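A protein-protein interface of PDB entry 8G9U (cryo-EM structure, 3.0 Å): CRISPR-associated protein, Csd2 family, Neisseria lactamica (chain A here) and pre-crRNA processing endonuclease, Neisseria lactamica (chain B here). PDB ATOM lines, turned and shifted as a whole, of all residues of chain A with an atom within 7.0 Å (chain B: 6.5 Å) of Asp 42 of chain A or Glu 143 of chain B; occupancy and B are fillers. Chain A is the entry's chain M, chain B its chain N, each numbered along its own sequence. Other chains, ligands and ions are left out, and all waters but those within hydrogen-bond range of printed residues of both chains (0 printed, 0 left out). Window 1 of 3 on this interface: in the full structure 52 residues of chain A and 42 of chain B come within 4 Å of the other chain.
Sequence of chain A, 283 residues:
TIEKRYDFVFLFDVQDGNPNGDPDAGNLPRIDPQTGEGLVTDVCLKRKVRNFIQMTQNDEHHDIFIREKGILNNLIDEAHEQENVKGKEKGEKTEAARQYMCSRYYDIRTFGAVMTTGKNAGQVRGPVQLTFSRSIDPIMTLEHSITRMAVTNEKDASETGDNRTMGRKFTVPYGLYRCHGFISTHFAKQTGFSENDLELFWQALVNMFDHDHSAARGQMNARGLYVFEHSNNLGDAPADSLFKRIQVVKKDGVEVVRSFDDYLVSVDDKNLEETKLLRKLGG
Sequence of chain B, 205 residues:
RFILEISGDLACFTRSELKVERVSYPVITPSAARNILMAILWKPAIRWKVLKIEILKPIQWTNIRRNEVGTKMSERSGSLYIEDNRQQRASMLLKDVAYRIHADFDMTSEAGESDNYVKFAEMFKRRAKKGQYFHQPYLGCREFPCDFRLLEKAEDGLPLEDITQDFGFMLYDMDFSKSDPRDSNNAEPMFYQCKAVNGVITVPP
Asp 42 of chain A touches one residue of chain B.
Glu 143 of chain B touches four residues of chain A.
Of the printed residues of chain B, Phe 132 of chain A touches Leu 10, Arg 66, Glu 143 and Phe 144.
Of the printed residues of chain B, Val 128 of chain A touches Arg 142.
Printed residues of chain A within 4 Å of Leu 10 of chain B: Phe 132.
Printed residues of chain B within 4 Å of Phe 111 of chain A: Arg 142 (3.9 Å).
The nearest residue of chain B that does not touch Asp 42 of chain A is Arg 142 of chain B (4.9 Å).
The nearest printed residue of chain B that does not touch Leu 130 of chain A is Phe 144 of chain B (4.5 Å).
The backbone carbonyl oxygen (O) of Leu 130 of chain A sits close to the backbone carbonyl oxygen (O) of Glu 143 of chain B (3.3 Å).
O of Glu 143 of chain B sits at hydrogen-bond distance from N of Phe 132 of chain A, at 3.5 Å.
NE2 of Gln 129 of chain A is in hydrogen-bond range of O of Arg 142 of chain B (3.1 Å).
O of Arg 142 of chain B lies close to O of Leu 130 of chain A (3.4 Å).
Printed residues of chain B that touch a printed residue of chain A: Leu 10, Arg 66, Arg 142, Glu 143, Phe 144 and Pro 145.
Hydrophobic or aromatic side chains of chain B that line the printed part of chain A: Leu 10, Phe 144 and Pro 145.
Along chain B the printed residues that touch a printed residue of chain A span positions 10 to 145.
Of the 22 printed residues of chain A, 10 touch a printed residue of chain B.
Printed residues of chain A that touch a printed residue of chain B: Thr 41, Asp 42, Val 43, Phe 111, Val 128, Gln 129, Leu 130, Thr 131, Phe 132 and Phe 182.
Along chain A the printed residues that touch a printed residue of chain B span positions 41 to 182.
Among the printed residues, 16 pairs touch across the chains.
Among the printed residues, no Asp or Glu carboxylate lies within 4 Å of a Lys or Arg side-chain nitrogen of the other chain.
N of Thr 131 of chain A is in hydrogen-bond range of O of His 180 of chain A (2.8 Å).
SG of Cys 179 of chain A lies within hydrogen-bond range of O of Thr 131 of chain A (3.2 Å).
The guanidinium group (NH1) of Arg 66 of chain B lies within salt-bridge range of the side-chain carboxylate (OE2) of Glu 68 of chain B, at 3.0 Å.
O of Gln 129 of chain A lies within hydrogen-bond range of N of Phe 182 of chain A, at 2.8 Å.
The side-chain amino group (NZ) of Lys 46 of chain A lies within salt-bridge range of the side-chain carboxylate (OD2) of Asp 42 of chain A, at 2.6 Å.
The side-chain amide nitrogen of Asn 20 of chain A sits at hydrogen-bond distance from the side-chain hydroxyl of Thr 41 of chain A (2.4 Å).
CG2 of Thr 41 of chain A touches CG of Arg 66 of chain B, at 3.5 Å.
CD of Arg 66 of chain B touches CG2 of Val 43 of chain A, at 3.9996 Å.
Val 128 of chain A touches Arg 142 of chain B (C to NH1, 3.5 Å).
NE2 of Gln 129 of chain A touches CA of Pro 145 of chain B, at 3.8 Å.
Thr 131 of chain A touches Glu 143 of chain B (CA to O, 3.7 Å).
Pro 145 of chain B touches Thr 131 of chain A.
Leu 10 of chain B touches Phe 132 of chain A (CD2 to CD2, 3.4 Å).
Arg 66 of chain B touches Phe 132 of chain A (NH2 to CZ, 3.1 Å).
CZ of Phe 132 of chain A touches CE1 of Phe 144 of chain B, 3.4 Å away.
Phe 182 of chain A touches Pro 145 of chain B.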
ATOM      1  N   ASN A  20     -12.171  31.790  30.251  1.00  0.00           N
ATOM      2  CA  ASN A  20     -13.340  31.013  29.889  1.00  0.00           C
ATOM      3  C   ASN A  20     -14.301  31.188  31.053  1.00  0.00           C
ATOM      4  O   ASN A  20     -14.132  30.548  32.089  1.00  0.00           O
ATOM      5  CB  ASN A  20     -12.976  29.558  29.693  1.00  0.00           C
ATOM      6  CG  ASN A  20     -13.912  28.862  28.787  1.00  0.00           C
ATOM      7  OD1 ASN A  20     -14.574  29.491  27.985  1.00  0.00           O
ATOM      8  ND2 ASN A  20     -14.002  27.554  28.914  1.00  0.00           N
ATOM      9  N   VAL A  40     -10.400  26.139  31.945  1.00  0.00           N
ATOM     10  CA  VAL A  40     -10.745  26.693  30.650  1.00  0.00           C
ATOM     11  C   VAL A  40     -11.126  25.499  29.802  1.00  0.00           C
ATOM     12  O   VAL A  40     -10.253  24.765  29.333  1.00  0.00           O
ATOM     13  CB  VAL A  40      -9.605  27.476  30.015  1.00  0.00           C
ATOM     14  CG1 VAL A  40      -9.994  27.892  28.640  1.00  0.00           C
ATOM     15  CG2 VAL A  40      -9.305  28.672  30.827  1.00  0.00           C
ATOM     16  N   THR A  41     -12.421  25.286  29.622  1.00  0.00           N
ATOM     17  CA  THR A  41     -12.877  24.123  28.887  1.00  0.00           C
ATOM     18  C   THR A  41     -12.224  24.089  27.523  1.00  0.00           C
ATOM     19  O   THR A  41     -12.118  25.108  26.844  1.00  0.00           O
ATOM     20  CB  THR A  41     -14.387  24.149  28.746  1.00  0.00           C
ATOM     21  OG1 THR A  41     -14.782  25.401  28.189  1.00  0.00           O
ATOM     22  CG2 THR A  41     -15.005  24.004  30.093  1.00  0.00           C
ATOM     23  N   ASP A  42     -11.758  22.906  27.141  1.00  0.00           N
ATOM     24  CA  ASP A  42     -11.013  22.775  25.904  1.00  0.00           C
ATOM     25  C   ASP A  42     -11.801  23.303  24.723  1.00  0.00           C
ATOM     26  O   ASP A  42     -11.209  23.770  23.748  1.00  0.00           O
ATOM     27  CB  ASP A  42     -10.664  21.319  25.675  1.00  0.00           C
ATOM     28  CG  ASP A  42     -11.882  20.476  25.491  1.00  0.00           C
ATOM     29  OD1 ASP A  42     -12.935  20.866  26.032  1.00  0.00           O
ATOM     30  OD2 ASP A  42     -11.797  19.441  24.802  1.00  0.00           O
ATOM     31  N   VAL A  43     -13.130  23.240  24.787  1.00  0.00           N
ATOM     32  CA  VAL A  43     -13.929  23.791  23.705  1.00  0.00           C
ATOM     33  C   VAL A  43     -13.646  25.273  23.541  1.00  0.00           C
ATOM     34  O   VAL A  43     -13.711  25.799  22.428  1.00  0.00           O
ATOM     35  CB  VAL A  43     -15.419  23.513  23.940  1.00  0.00           C
ATOM     36  CG1 VAL A  43     -15.668  22.031  23.917  1.00  0.00           C
ATOM     37  CG2 VAL A  43     -15.826  24.055  25.256  1.00  0.00           C
ATOM     38  N   CYS A  44     -13.297  25.964  24.626  1.00  0.00           N
ATOM     39  CA  CYS A  44     -12.810  27.332  24.490  1.00  0.00           C
ATOM     40  C   CYS A  44     -11.506  27.362  23.710  1.00  0.00           C
ATOM     41  O   CYS A  44     -11.352  28.141  22.767  1.00  0.00           O
ATOM     42  CB  CYS A  44     -12.625  27.966  25.861  1.00  0.00           C
ATOM     43  SG  CYS A  44     -11.902  29.601  25.838  1.00  0.00           S
ATOM     44  N   LEU A  45     -10.553  26.515  24.090  1.00  0.00           N
ATOM     45  CA  LEU A  45      -9.344  26.370  23.292  1.00  0.00           C
ATOM     46  C   LEU A  45      -9.688  25.867  21.905  1.00  0.00           C
ATOM     47  O   LEU A  45      -9.193  26.387  20.903  1.00  0.00           O
ATOM     48  CB  LEU A  45      -8.379  25.400  23.960  1.00  0.00           C
ATOM     49  CG  LEU A  45      -7.450  25.875  25.061  1.00  0.00           C
ATOM     50  CD1 LEU A  45      -6.500  26.879  24.542  1.00  0.00           C
ATOM     51  CD2 LEU A  45      -8.244  26.473  26.150  1.00  0.00           C
ATOM     52  N   LYS A  46     -10.548  24.860  21.826  1.00  0.00           N
ATOM     53  CA  LYS A  46     -11.009  24.378  20.539  1.00  0.00           C
ATOM     54  C   LYS A  46     -11.727  25.454  19.753  1.00  0.00           C
ATOM     55  O   LYS A  46     -11.821  25.345  18.529  1.00  0.00           O
ATOM     56  CB  LYS A  46     -11.924  23.177  20.739  1.00  0.00           C
ATOM     57  CG  LYS A  46     -11.201  21.907  21.108  1.00  0.00           C
ATOM     58  CD  LYS A  46     -12.126  20.893  21.733  1.00  0.00           C
ATOM     59  CE  LYS A  46     -11.516  19.514  21.701  1.00  0.00           C
ATOM     60  NZ  LYS A  46     -12.336  18.530  22.445  1.00  0.00           N
ATOM     61  N   ARG A  47     -12.224  26.486  20.419  1.00  0.00           N
ATOM     62  CA  ARG A  47     -12.820  27.625  19.751  1.00  0.00           C
ATOM     63  C   ARG A  47     -11.777  28.572  19.201  1.00  0.00           C
ATOM     64  O   ARG A  47     -11.848  28.943  18.030  1.00  0.00           O
ATOM     65  CB  ARG A  47     -13.740  28.360  20.714  1.00  0.00           C
ATOM     66  CG  ARG A  47     -14.355  29.620  20.201  1.00  0.00           C
ATOM     67  CD  ARG A  47     -14.748  29.489  18.774  1.00  0.00           C
ATOM     68  NE  ARG A  47     -15.761  28.487  18.539  1.00  0.00           N
ATOM     69  CZ  ARG A  47     -16.094  28.081  17.328  1.00  0.00           C
ATOM     70  NH1 ARG A  47     -15.493  28.593  16.271  1.00  0.00           N
ATOM     71  NH2 ARG A  47     -17.024  27.168  17.172  1.00  0.00           N
ATOM     72  N   LYS A  48     -10.797  28.936  19.984  1.00  0.00           N
ATOM     73  CA  LYS A  48      -9.812  29.871  19.496  1.00  0.00           C
ATOM     74  C   LYS A  48      -8.919  29.284  18.424  1.00  0.00           C
ATOM     75  O   LYS A  48      -8.491  30.016  17.537  1.00  0.00           O
ATOM     76  CB  LYS A  48      -8.984  30.386  20.665  1.00  0.00           C
ATOM     77  CG  LYS A  48      -9.869  30.873  21.764  1.00  0.00           C
ATOM     78  CD  LYS A  48      -9.169  31.825  22.666  1.00  0.00           C
ATOM     79  CE  LYS A  48      -9.858  31.823  23.990  1.00  0.00           C
ATOM     80  NZ  LYS A  48     -11.322  31.939  23.771  1.00  0.00           N
ATOM     81  N   VAL A  49      -8.647  27.984  18.462  1.00  0.00           N
ATOM     82  CA  VAL A  49      -8.098  27.326  17.286  1.00  0.00           C
ATOM     83  C   VAL A  49      -9.066  27.447  16.128  1.00  0.00           C
ATOM     84  O   VAL A  49      -8.676  27.776  15.006  1.00  0.00           O
ATOM     85  CB  VAL A  49      -7.780  25.855  17.583  1.00  0.00           C
ATOM     86  CG1 VAL A  49      -7.066  25.238  16.414  1.00  0.00           C
ATOM     87  CG2 VAL A  49      -6.951  25.737  18.825  1.00  0.00           C
ATOM     88  N   ARG A  50     -10.346  27.183  16.377  1.00  0.00           N
ATOM     89  CA  ARG A  50     -11.339  27.335  15.325  1.00  0.00           C
ATOM     90  C   ARG A  50     -11.367  28.763  14.826  1.00  0.00           C
ATOM     91  O   ARG A  50     -11.361  29.016  13.617  1.00  0.00           O
ATOM     92  CB  ARG A  50     -12.713  26.950  15.844  1.00  0.00           C
ATOM     93  CG  ARG A  50     -13.043  25.514  15.714  1.00  0.00           C
ATOM     94  CD  ARG A  50     -14.464  25.310  16.113  1.00  0.00           C
ATOM     95  NE  ARG A  50     -14.812  23.914  16.016  1.00  0.00           N
ATOM     96  CZ  ARG A  50     -14.544  23.039  16.964  1.00  0.00           C
ATOM     97  NH1 ARG A  50     -13.923  23.433  18.062  1.00  0.00           N
ATOM     98  NH2 ARG A  50     -14.880  21.772  16.800  1.00  0.00           N
ATOM     99  N   PHE A 111     -10.466  18.940  14.914  1.00  0.00           N
ATOM    100  CA  PHE A 111     -11.140  18.625  16.157  1.00  0.00           C
ATOM    101  C   PHE A 111     -12.172  17.531  16.010  1.00  0.00           C
ATOM    102  O   PHE A 111     -12.674  17.041  17.021  1.00  0.00           O
ATOM    103  CB  PHE A 111     -11.786  19.879  16.717  1.00  0.00           C
ATOM    104  CG  PHE A 111     -10.797  20.870  17.201  1.00  0.00           C
ATOM    105  CD1 PHE A 111      -9.881  20.518  18.158  1.00  0.00           C
ATOM    106  CD2 PHE A 111     -10.758  22.137  16.682  1.00  0.00           C
ATOM    107  CE1 PHE A 111      -8.956  21.414  18.598  1.00  0.00           C
ATOM    108  CE2 PHE A 111      -9.841  23.036  17.123  1.00  0.00           C
ATOM    109  CZ  PHE A 111      -8.937  22.673  18.083  1.00  0.00           C
ATOM    110  N   VAL A 128      -7.319  15.781  17.082  1.00  0.00           N
ATOM    111  CA  VAL A 128      -6.985  16.684  18.170  1.00  0.00           C
ATOM    112  C   VAL A 128      -8.005  16.512  19.286  1.00  0.00           C
ATOM    113  O   VAL A 128      -9.092  17.086  19.254  1.00  0.00           O
ATOM    114  CB  VAL A 128      -6.920  18.129  17.703  1.00  0.00           C
ATOM    115  CG1 VAL A 128      -6.528  18.973  18.864  1.00  0.00           C
ATOM    116  CG2 VAL A 128      -5.927  18.244  16.597  1.00  0.00           C
ATOM    117  N   GLN A 129      -7.642  15.724  20.279  1.00  0.00           N
ATOM    118  CA  GLN A 129      -8.338  15.730  21.548  1.00  0.00           C
ATOM    119  C   GLN A 129      -7.699  16.790  22.424  1.00  0.00           C
ATOM    120  O   GLN A 129      -6.519  17.098  22.280  1.00  0.00           O
ATOM    121  CB  GLN A 129      -8.262  14.357  22.201  1.00  0.00           C
ATOM    122  CG  GLN A 129      -8.766  14.307  23.607  1.00  0.00           C
ATOM    123  CD  GLN A 129      -8.576  12.956  24.202  1.00  0.00           C
ATOM    124  OE1 GLN A 129      -8.455  11.972  23.480  1.00  0.00           O
ATOM    125  NE2 GLN A 129      -8.548  12.887  25.523  1.00  0.00           N
ATOM    126  N   LEU A 130      -8.488  17.372  23.313  1.00  0.00           N
ATOM    127  CA  LEU A 130      -8.004  18.498  24.086  1.00  0.00           C
ATOM    128  C   LEU A 130      -8.480  18.365  25.522  1.00  0.00           C
ATOM    129  O   LEU A 130      -9.498  17.732  25.798  1.00  0.00           O
ATOM    130  CB  LEU A 130      -8.475  19.806  23.459  1.00  0.00           C
ATOM    131  CG  LEU A 130      -7.534  20.988  23.567  1.00  0.00           C
ATOM    132  CD1 LEU A 130      -6.232  20.579  22.997  1.00  0.00           C
ATOM    133  CD2 LEU A 130      -8.064  22.129  22.775  1.00  0.00           C
ATOM    134  N   THR A 131      -7.730  18.962  26.434  1.00  0.00           N
ATOM    135  CA  THR A 131      -7.986  18.852  27.858  1.00  0.00           C
ATOM    136  C   THR A 131      -8.549  20.163  28.379  1.00  0.00           C
ATOM    137  O   THR A 131      -8.178  21.240  27.912  1.00  0.00           O
ATOM    138  CB  THR A 131      -6.700  18.517  28.610  1.00  0.00           C
ATOM    139  OG1 THR A 131      -6.186  17.274  28.130  1.00  0.00           O
ATOM    140  CG2 THR A 131      -6.936  18.411  30.104  1.00  0.00           C
ATOM    141  N   PHE A 132      -9.461  20.065  29.335  1.00  0.00           N
ATOM    142  CA  PHE A 132      -9.861  21.247  30.076  1.00  0.00           C
ATOM    143  C   PHE A 132      -8.631  21.936  30.621  1.00  0.00           C
ATOM    144  O   PHE A 132      -7.893  21.368  31.428  1.00  0.00           O
ATOM    145  CB  PHE A 132     -10.796  20.872  31.214  1.00  0.00           C
ATOM    146  CG  PHE A 132     -12.211  20.748  30.806  1.00  0.00           C
ATOM    147  CD1 PHE A 132     -12.543  20.488  29.502  1.00  0.00           C
ATOM    148  CD2 PHE A 132     -13.213  20.896  31.728  1.00  0.00           C
ATOM    149  CE1 PHE A 132     -13.847  20.376  29.132  1.00  0.00           C
ATOM    150  CE2 PHE A 132     -14.514  20.779  31.364  1.00  0.00           C
ATOM    151  CZ  PHE A 132     -14.834  20.517  30.066  1.00  0.00           C
ATOM    152  N   SER A 133      -8.408  23.160  30.180  1.00  0.00           N
ATOM    153  CA  SER A 133      -7.167  23.827  30.509  1.00  0.00           C
ATOM    154  C   SER A 133      -7.161  24.265  31.959  1.00  0.00           C
ATOM    155  O   SER A 133      -7.525  25.399  32.267  1.00  0.00           O
ATOM    156  CB  SER A 133      -6.976  25.026  29.603  1.00  0.00           C
ATOM    157  OG  SER A 133      -6.846  24.615  28.260  1.00  0.00           O
ATOM    158  N   CYS A 179      -3.105  23.144  29.218  1.00  0.00           N
ATOM    159  CA  CYS A 179      -3.961  22.285  28.425  1.00  0.00           C
ATOM    160  C   CYS A 179      -3.146  21.107  27.932  1.00  0.00           C
ATOM    161  O   CYS A 179      -1.952  21.242  27.682  1.00  0.00           O
ATOM    162  CB  CYS A 179      -4.518  23.041  27.237  1.00  0.00           C
ATOM    163  SG  CYS A 179      -5.596  22.093  26.196  1.00  0.00           S
ATOM    164  N   HIS A 180      -3.779  19.956  27.792  1.00  0.00           N
ATOM    165  CA  HIS A 180      -3.134  18.790  27.213  1.00  0.00           C
ATOM    166  C   HIS A 180      -3.926  18.339  26.002  1.00  0.00           C
ATOM    167  O   HIS A 180      -5.100  17.990  26.118  1.00  0.00           O
ATOM    168  CB  HIS A 180      -3.032  17.646  28.217  1.00  0.00           C
ATOM    169  CG  HIS A 180      -2.328  18.011  29.480  1.00  0.00           C
ATOM    170  ND1 HIS A 180      -2.639  17.440  30.692  1.00  0.00           N
ATOM    171  CD2 HIS A 180      -1.330  18.888  29.721  1.00  0.00           C
ATOM    172  CE1 HIS A 180      -1.862  17.951  31.628  1.00  0.00           C
ATOM    173  NE2 HIS A 180      -1.058  18.833  31.065  1.00  0.00           N
ATOM    174  N   PHE A 182      -4.039  15.765  22.487  1.00  0.00           N
ATOM    175  CA  PHE A 182      -3.584  14.446  22.066  1.00  0.00           C
ATOM    176  C   PHE A 182      -3.901  14.302  20.593  1.00  0.00           C
ATOM    177  O   PHE A 182      -4.926  13.723  20.241  1.00  0.00           O
ATOM    178  CB  PHE A 182      -4.270  13.391  22.854  1.00  0.00           C
ATOM    179  CG  PHE A 182      -4.206  13.596  24.318  1.00  0.00           C
ATOM    180  CD1 PHE A 182      -3.135  13.163  25.043  1.00  0.00           C
ATOM    181  CD2 PHE A 182      -5.233  14.233  24.969  1.00  0.00           C
ATOM    182  CE1 PHE A 182      -3.099  13.351  26.383  1.00  0.00           C
ATOM    183  CE2 PHE A 182      -5.189  14.426  26.307  1.00  0.00           C
ATOM    184  CZ  PHE A 182      -4.121  13.986  27.017  1.00  0.00           C
ATOM    185  N   LEU B  10     -10.827  15.143  35.333  1.00  0.00           N
ATOM    186  CA  LEU B  10     -12.267  15.263  35.194  1.00  0.00           C
ATOM    187  C   LEU B  10     -12.780  14.095  34.369  1.00  0.00           C
ATOM    188  O   LEU B  10     -12.026  13.454  33.637  1.00  0.00           O
ATOM    189  CB  LEU B  10     -12.663  16.586  34.535  1.00  0.00           C
ATOM    190  CG  LEU B  10     -13.131  17.741  35.418  1.00  0.00           C
ATOM    191  CD1 LEU B  10     -12.176  17.992  36.544  1.00  0.00           C
ATOM    192  CD2 LEU B  10     -13.247  18.988  34.594  1.00  0.00           C
ATOM    193  N   ARG B  22     -25.509  17.442  31.112  1.00  0.00           N
ATOM    194  CA  ARG B  22     -24.706  16.271  31.433  1.00  0.00           C
ATOM    195  C   ARG B  22     -24.504  16.101  32.926  1.00  0.00           C
ATOM    196  O   ARG B  22     -23.974  16.980  33.604  1.00  0.00           O
ATOM    197  CB  ARG B  22     -23.348  16.385  30.735  1.00  0.00           C
ATOM    198  CG  ARG B  22     -23.395  16.126  29.242  1.00  0.00           C
ATOM    199  CD  ARG B  22     -22.114  16.540  28.540  1.00  0.00           C
ATOM    200  NE  ARG B  22     -22.174  16.264  27.107  1.00  0.00           N
ATOM    201  CZ  ARG B  22     -21.988  15.063  26.566  1.00  0.00           C
ATOM    202  NH1 ARG B  22     -21.725  14.016  27.333  1.00  0.00           N
ATOM    203  NH2 ARG B  22     -22.067  14.900  25.256  1.00  0.00           N
ATOM    204  N   ARG B  66     -20.914  24.153  29.795  1.00  0.00           N
ATOM    205  CA  ARG B  66     -20.202  24.528  28.595  1.00  0.00           C
ATOM    206  C   ARG B  66     -21.198  24.950  27.535  1.00  0.00           C
ATOM    207  O   ARG B  66     -22.260  24.337  27.382  1.00  0.00           O
ATOM    208  CB  ARG B  66     -19.369  23.361  28.091  1.00  0.00           C
ATOM    209  CG  ARG B  66     -18.142  23.093  28.892  1.00  0.00           C
ATOM    210  CD  ARG B  66     -17.338  21.951  28.303  1.00  0.00           C
ATOM    211  NE  ARG B  66     -18.153  20.793  27.961  1.00  0.00           N
ATOM    212  CZ  ARG B  66     -18.390  19.781  28.786  1.00  0.00           C
ATOM    213  NH1 ARG B  66     -19.143  18.767  28.393  1.00  0.00           N
ATOM    214  NH2 ARG B  66     -17.877  19.782  30.003  1.00  0.00           N
ATOM    215  N   GLU B  68     -22.241  24.277  24.655  1.00  0.00           N
ATOM    216  CA  GLU B  68     -22.116  23.179  23.728  1.00  0.00           C
ATOM    217  C   GLU B  68     -22.854  23.637  22.468  1.00  0.00           C
ATOM    218  O   GLU B  68     -23.513  24.681  22.461  1.00  0.00           O
ATOM    219  CB  GLU B  68     -22.713  21.941  24.376  1.00  0.00           C
ATOM    220  CG  GLU B  68     -21.992  21.423  25.667  1.00  0.00           C
ATOM    221  CD  GLU B  68     -20.590  20.881  25.540  1.00  0.00           C
ATOM    222  OE1 GLU B  68     -20.235  20.318  24.517  1.00  0.00           O
ATOM    223  OE2 GLU B  68     -19.840  20.944  26.522  1.00  0.00           O
ATOM    224  N   TYR B 138     -10.888   8.388  26.390  1.00  0.00           N
ATOM    225  CA  TYR B 138     -11.861   9.387  26.779  1.00  0.00           C
ATOM    226  C   TYR B 138     -12.548   8.910  28.051  1.00  0.00           C
ATOM    227  O   TYR B 138     -13.127   7.820  28.081  1.00  0.00           O
ATOM    228  CB  TYR B 138     -12.861   9.621  25.645  1.00  0.00           C
ATOM    229  CG  TYR B 138     -13.911   8.536  25.484  1.00  0.00           C
ATOM    230  CD1 TYR B 138     -13.591   7.278  25.001  1.00  0.00           C
ATOM    231  CD2 TYR B 138     -15.227   8.776  25.826  1.00  0.00           C
ATOM    232  CE1 TYR B 138     -14.556   6.306  24.867  1.00  0.00           C
ATOM    233  CE2 TYR B 138     -16.194   7.807  25.699  1.00  0.00           C
ATOM    234  CZ  TYR B 138     -15.861   6.581  25.216  1.00  0.00           C
ATOM    235  OH  TYR B 138     -16.863   5.656  25.092  1.00  0.00           O
ATOM    236  N   GLY B 140     -15.358   9.096  29.276  1.00  0.00           N
ATOM    237  CA  GLY B 140     -16.721   9.463  28.940  1.00  0.00           C
ATOM    238  C   GLY B 140     -16.829  10.535  27.896  1.00  0.00           C
ATOM    239  O   GLY B 140     -17.622  10.406  26.960  1.00  0.00           O
ATOM    240  N   CYS B 141     -16.045  11.599  28.022  1.00  0.00           N
ATOM    241  CA  CYS B 141     -16.000  12.664  27.033  1.00  0.00           C
ATOM    242  C   CYS B 141     -14.555  12.997  26.702  1.00  0.00           C
ATOM    243  O   CYS B 141     -13.730  13.160  27.604  1.00  0.00           O
ATOM    244  CB  CYS B 141     -16.720  13.902  27.540  1.00  0.00           C
ATOM    245  SG  CYS B 141     -18.484  13.697  27.802  1.00  0.00           S
ATOM    246  N   ARG B 142     -14.255  13.124  25.406  1.00  0.00           N
ATOM    247  CA  ARG B 142     -12.874  13.345  24.987  1.00  0.00           C
ATOM    248  C   ARG B 142     -12.265  14.581  25.610  1.00  0.00           C
ATOM    249  O   ARG B 142     -11.043  14.659  25.744  1.00  0.00           O
ATOM    250  CB  ARG B 142     -12.762  13.469  23.479  1.00  0.00           C
ATOM    251  CG  ARG B 142     -13.068  12.233  22.725  1.00  0.00           C
ATOM    252  CD  ARG B 142     -12.920  12.567  21.277  1.00  0.00           C
ATOM    253  NE  ARG B 142     -11.538  12.871  20.943  1.00  0.00           N
ATOM    254  CZ  ARG B 142     -11.165  13.355  19.772  1.00  0.00           C
ATOM    255  NH1 ARG B 142      -9.894  13.607  19.520  1.00  0.00           N
ATOM    256  NH2 ARG B 142     -12.076  13.602  18.854  1.00  0.00           N
ATOM    257  N   GLU B 143     -13.079  15.561  25.985  1.00  0.00           N
ATOM    258  CA  GLU B 143     -12.532  16.691  26.716  1.00  0.00           C
ATOM    259  C   GLU B 143     -11.805  16.256  27.980  1.00  0.00           C
ATOM    260  O   GLU B 143     -11.137  17.080  28.609  1.00  0.00           O
ATOM    261  CB  GLU B 143     -13.645  17.676  27.073  1.00  0.00           C
ATOM    262  CG  GLU B 143     -14.432  18.228  25.897  1.00  0.00           C
ATOM    263  CD  GLU B 143     -15.532  17.312  25.429  1.00  0.00           C
ATOM    264  OE1 GLU B 143     -15.683  16.244  26.038  1.00  0.00           O
ATOM    265  OE2 GLU B 143     -16.244  17.658  24.457  1.00  0.00           O
ATOM    266  N   PHE B 144     -11.916  14.988  28.354  1.00  0.00           N
ATOM    267  CA  PHE B 144     -11.352  14.466  29.593  1.00  0.00           C
ATOM    268  C   PHE B 144     -10.431  13.299  29.290  1.00  0.00           C
ATOM    269  O   PHE B 144     -10.885  12.279  28.740  1.00  0.00           O
ATOM    270  CB  PHE B 144     -12.487  14.051  30.517  1.00  0.00           C
ATOM    271  CG  PHE B 144     -13.531  15.104  30.653  1.00  0.00           C
ATOM    272  CD1 PHE B 144     -13.187  16.376  31.043  1.00  0.00           C
ATOM    273  CD2 PHE B 144     -14.838  14.847  30.333  1.00  0.00           C
ATOM    274  CE1 PHE B 144     -14.131  17.348  31.152  1.00  0.00           C
ATOM    275  CE2 PHE B 144     -15.781  15.826  30.437  1.00  0.00           C
ATOM    276  CZ  PHE B 144     -15.426  17.073  30.846  1.00  0.00           C
ATOM    277  N   PRO B 145      -9.146  13.409  29.591  1.00  0.00           N
ATOM    278  CA  PRO B 145      -8.198  12.354  29.243  1.00  0.00           C
ATOM    279  C   PRO B 145      -8.013  11.353  30.365  1.00  0.00           C
ATOM    280  O   PRO B 145      -8.089  11.676  31.549  1.00  0.00           O
ATOM    281  CB  PRO B 145      -6.897  13.132  29.013  1.00  0.00           C
ATOM    282  CG  PRO B 145      -7.286  14.574  29.031  1.00  0.00           C
ATOM    283  CD  PRO B 145      -8.451  14.652  29.925  1.00  0.00           C
